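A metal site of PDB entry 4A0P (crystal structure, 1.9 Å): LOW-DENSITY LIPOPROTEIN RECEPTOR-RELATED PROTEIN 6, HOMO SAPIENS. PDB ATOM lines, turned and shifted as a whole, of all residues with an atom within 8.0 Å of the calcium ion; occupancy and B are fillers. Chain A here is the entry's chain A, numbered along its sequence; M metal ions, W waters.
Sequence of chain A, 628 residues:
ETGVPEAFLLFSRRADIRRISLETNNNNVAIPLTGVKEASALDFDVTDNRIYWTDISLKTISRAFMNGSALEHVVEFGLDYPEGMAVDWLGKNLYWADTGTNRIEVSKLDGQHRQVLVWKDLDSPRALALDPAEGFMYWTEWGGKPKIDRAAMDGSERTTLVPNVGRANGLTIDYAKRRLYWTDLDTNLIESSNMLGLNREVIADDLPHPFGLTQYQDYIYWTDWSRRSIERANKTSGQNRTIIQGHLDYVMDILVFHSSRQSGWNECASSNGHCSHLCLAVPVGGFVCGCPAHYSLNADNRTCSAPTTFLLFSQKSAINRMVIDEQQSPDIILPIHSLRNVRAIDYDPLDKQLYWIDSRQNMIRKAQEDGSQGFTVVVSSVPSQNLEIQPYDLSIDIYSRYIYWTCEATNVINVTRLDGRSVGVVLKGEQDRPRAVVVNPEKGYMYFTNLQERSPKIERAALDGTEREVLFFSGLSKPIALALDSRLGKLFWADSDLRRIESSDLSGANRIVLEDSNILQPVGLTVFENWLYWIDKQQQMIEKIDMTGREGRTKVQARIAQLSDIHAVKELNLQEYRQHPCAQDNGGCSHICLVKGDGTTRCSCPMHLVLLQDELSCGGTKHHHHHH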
ATOM      1  N   ARG A 167      25.152 -29.136  33.639  1.00  0.00           N
ATOM      2  CA  ARG A 167      24.535 -28.641  34.864  1.00  0.00           C
ATOM      3  C   ARG A 167      23.030 -28.879  34.783  1.00  0.00           C
ATOM      4  O   ARG A 167      22.328 -28.299  33.943  1.00  0.00           O
ATOM      5  CB  ARG A 167      24.839 -27.155  35.067  1.00  0.00           C
ATOM      6  CG  ARG A 167      26.324 -26.874  35.323  1.00  0.00           C
ATOM      7  CD  ARG A 167      26.596 -25.391  35.394  1.00  0.00           C
ATOM      8  NE  ARG A 167      26.232 -24.717  34.152  1.00  0.00           N
ATOM      9  CZ  ARG A 167      25.849 -23.447  34.046  1.00  0.00           C
ATOM     10  NH1 ARG A 167      25.751 -22.665  35.115  1.00  0.00           N
ATOM     11  NH2 ARG A 167      25.537 -22.949  32.848  1.00  0.00           N
ATOM     12  N   ASP A 184      18.817 -29.515  31.440  1.00  0.00           N
ATOM     13  CA  ASP A 184      20.257 -29.429  31.269  1.00  0.00           C
ATOM     14  C   ASP A 184      20.544 -28.037  30.719  1.00  0.00           C
ATOM     15  O   ASP A 184      20.203 -27.724  29.570  1.00  0.00           O
ATOM     16  CB  ASP A 184      20.770 -30.534  30.353  1.00  0.00           C
ATOM     17  CG  ASP A 184      22.296 -30.625  30.313  1.00  0.00           C
ATOM     18  OD1 ASP A 184      22.970 -29.576  30.392  1.00  0.00           O
ATOM     19  OD2 ASP A 184      22.817 -31.753  30.181  1.00  0.00           O
ATOM     20  N   LEU A 185      21.169 -27.221  31.568  1.00  0.00           N
ATOM     21  CA  LEU A 185      21.469 -25.830  31.248  1.00  0.00           C
ATOM     22  C   LEU A 185      22.530 -25.694  30.172  1.00  0.00           C
ATOM     23  O   LEU A 185      22.582 -24.670  29.504  1.00  0.00           O
ATOM     24  CB  LEU A 185      21.923 -25.073  32.502  1.00  0.00           C
ATOM     25  CG  LEU A 185      20.948 -25.012  33.675  1.00  0.00           C
ATOM     26  CD1 LEU A 185      21.574 -24.233  34.832  1.00  0.00           C
ATOM     27  CD2 LEU A 185      19.629 -24.384  33.246  1.00  0.00           C
ATOM     28  N   ASP A 186      23.375 -26.712  29.999  1.00  0.00           N
ATOM     29  CA  ASP A 186      24.485 -26.614  29.041  1.00  0.00           C
ATOM     30  C   ASP A 186      24.149 -27.242  27.698  1.00  0.00           C
ATOM     31  O   ASP A 186      24.499 -26.696  26.663  1.00  0.00           O
ATOM     32  CB  ASP A 186      25.735 -27.266  29.643  1.00  0.00           C
ATOM     33  CG  ASP A 186      26.123 -26.647  30.971  1.00  0.00           C
ATOM     34  OD1 ASP A 186      26.195 -25.399  31.041  1.00  0.00           O
ATOM     35  OD2 ASP A 186      26.369 -27.397  31.939  1.00  0.00           O
ATOM     36  N   THR A 187      23.481 -28.386  27.718  1.00  0.00           N
ATOM     37  CA  THR A 187      23.068 -29.044  26.472  1.00  0.00           C
ATOM     38  C   THR A 187      21.767 -28.426  25.920  1.00  0.00           C
ATOM     39  O   THR A 187      21.398 -28.657  24.777  1.00  0.00           O
ATOM     40  CB  THR A 187      22.973 -30.575  26.644  1.00  0.00           C
ATOM     41  OG1 THR A 187      21.843 -30.927  27.446  1.00  0.00           O
ATOM     42  CG2 THR A 187      24.238 -31.127  27.315  1.00  0.00           C
ATOM     43  N   ASN A 188      21.102 -27.615  26.757  1.00  0.00           N
ATOM     44  CA  ASN A 188      19.941 -26.790  26.358  1.00  0.00           C
ATOM     45  C   ASN A 188      18.702 -27.601  26.058  1.00  0.00           C
ATOM     46  O   ASN A 188      18.065 -27.447  24.996  1.00  0.00           O
ATOM     47  CB  ASN A 188      20.288 -25.875  25.175  1.00  0.00           C
ATOM     48  CG  ASN A 188      21.418 -24.932  25.498  1.00  0.00           C
ATOM     49  OD1 ASN A 188      21.522 -24.436  26.614  1.00  0.00           O
ATOM     50  ND2 ASN A 188      22.287 -24.692  24.520  1.00  0.00           N
ATOM     51  N   LEU A 189      18.338 -28.454  27.001  1.00  0.00           N
ATOM     52  CA  LEU A 189      17.234 -29.387  26.796  1.00  0.00           C
ATOM     53  C   LEU A 189      16.643 -29.906  28.095  1.00  0.00           C
ATOM     54  O   LEU A 189      17.172 -29.669  29.187  1.00  0.00           O
ATOM     55  CB  LEU A 189      17.698 -30.547  25.917  1.00  0.00           C
ATOM     56  CG  LEU A 189      18.911 -31.367  26.364  1.00  0.00           C
ATOM     57  CD1 LEU A 189      18.537 -32.364  27.457  1.00  0.00           C
ATOM     58  CD2 LEU A 189      19.528 -32.084  25.170  1.00  0.00           C
ATOM     59  N   LEU A 207      16.380 -25.016  24.268  1.00  0.00           N
ATOM     60  CA  LEU A 207      16.040 -24.238  25.467  1.00  0.00           C
ATOM     61  C   LEU A 207      17.341 -23.749  26.097  1.00  0.00           C
ATOM     62  O   LEU A 207      18.012 -24.516  26.757  1.00  0.00           O
ATOM     63  CB  LEU A 207      15.268 -25.116  26.461  1.00  0.00           C
ATOM     64  CG  LEU A 207      13.849 -25.528  26.048  1.00  0.00           C
ATOM     65  CD1 LEU A 207      13.295 -26.596  26.989  1.00  0.00           C
ATOM     66  CD2 LEU A 207      12.938 -24.309  25.981  1.00  0.00           C
ATOM     67  N   PRO A 208      17.704 -22.469  25.874  1.00  0.00           N
ATOM     68  CA  PRO A 208      19.017 -21.988  26.334  1.00  0.00           C
ATOM     69  C   PRO A 208      19.280 -22.081  27.834  1.00  0.00           C
ATOM     70  O   PRO A 208      20.448 -22.201  28.245  1.00  0.00           O
ATOM     71  CB  PRO A 208      19.030 -20.530  25.881  1.00  0.00           C
ATOM     72  CG  PRO A 208      18.105 -20.480  24.734  1.00  0.00           C
ATOM     73  CD  PRO A 208      17.013 -21.451  25.067  1.00  0.00           C
ATOM     74  N   HIS A 209      18.235 -22.005  28.652  1.00  0.00           N
ATOM     75  CA  HIS A 209      18.409 -22.033  30.106  1.00  0.00           C
ATOM     76  C   HIS A 209      17.124 -22.489  30.805  1.00  0.00           C
ATOM     77  O   HIS A 209      16.467 -21.691  31.486  1.00  0.00           O
ATOM     78  CB  HIS A 209      18.841 -20.650  30.589  1.00  0.00           C
ATOM     79  CG  HIS A 209      19.591 -20.668  31.894  1.00  0.00           C
ATOM     80  ND1 HIS A 209      20.935 -20.956  31.968  1.00  0.00           N
ATOM     81  CD2 HIS A 209      19.186 -20.406  33.158  1.00  0.00           C
ATOM     82  CE1 HIS A 209      21.325 -20.879  33.228  1.00  0.00           C
ATOM     83  NE2 HIS A 209      20.288 -20.547  33.971  1.00  0.00           N
ATOM     84  N   PRO A 210      16.753 -23.768  30.635  1.00  0.00           N
ATOM     85  CA  PRO A 210      15.598 -24.325  31.336  1.00  0.00           C
ATOM     86  C   PRO A 210      15.938 -24.550  32.806  1.00  0.00           C
ATOM     87  O   PRO A 210      16.597 -25.536  33.151  1.00  0.00           O
ATOM     88  CB  PRO A 210      15.366 -25.652  30.608  1.00  0.00           C
ATOM     89  CG  PRO A 210      16.711 -26.055  30.112  1.00  0.00           C
ATOM     90  CD  PRO A 210      17.487 -24.785  29.868  1.00  0.00           C
ATOM     91  N   ASP A 224      12.112 -21.326  31.254  1.00  0.00           N
ATOM     92  CA  ASP A 224      13.382 -21.015  30.638  1.00  0.00           C
ATOM     93  C   ASP A 224      13.620 -19.518  30.787  1.00  0.00           C
ATOM     94  O   ASP A 224      12.774 -18.717  30.411  1.00  0.00           O
ATOM     95  CB  ASP A 224      13.371 -21.421  29.170  1.00  0.00           C
ATOM     96  CG  ASP A 224      14.723 -21.213  28.495  1.00  0.00           C
ATOM     97  OD1 ASP A 224      15.094 -20.044  28.264  1.00  0.00           O
ATOM     98  OD2 ASP A 224      15.399 -22.218  28.190  1.00  0.00           O
HETATM   99 CA    CA M   1      22.577 -22.894  27.977  1.00  0.00          CA
HETATM  100  O   HOH W   1      22.655 -21.311  26.165  1.00  0.00           O
HETATM  101  O   HOH W   2      24.208 -23.855  26.733  1.00  0.00           O
HETATM  102  O   HOH W   3      24.768 -22.091  28.715  1.00  0.00           O
HETATM  103  O   HOH W   4      22.571 -21.421  29.871  1.00  0.00           O
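Of the 12 residues printed, 3 come within 4 Å of the calcium ion.
The backbone carbonyl oxygen of Asn 188 is in hydrogen-bond range of the backbone NH of Leu 207 (3.0 Å).
O of Arg 167 sits at hydrogen-bond distance from N of Leu 185 (2.9 Å).
O of Pro 208 binds the calcium ion, at 2.3 Å.
The calcium ion is bound by water W2, 2.3 Å away.
The calcium ion is bound by the side-chain amide oxygen (OD1) of Asn 188 (2.3 Å).
O of Leu 185 binds the calcium ion.
Water W4 is bound to the calcium ion, 2.4 Å away.
Water W1 binds the calcium ion, 2.4 Å away.
Water W3 binds the calcium ion, 2.4 Å away.
Water W2 bridges the backbone carbonyl oxygen (O) of Asp 186 and the side-chain amide nitrogen (ND2) of Asn 188.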
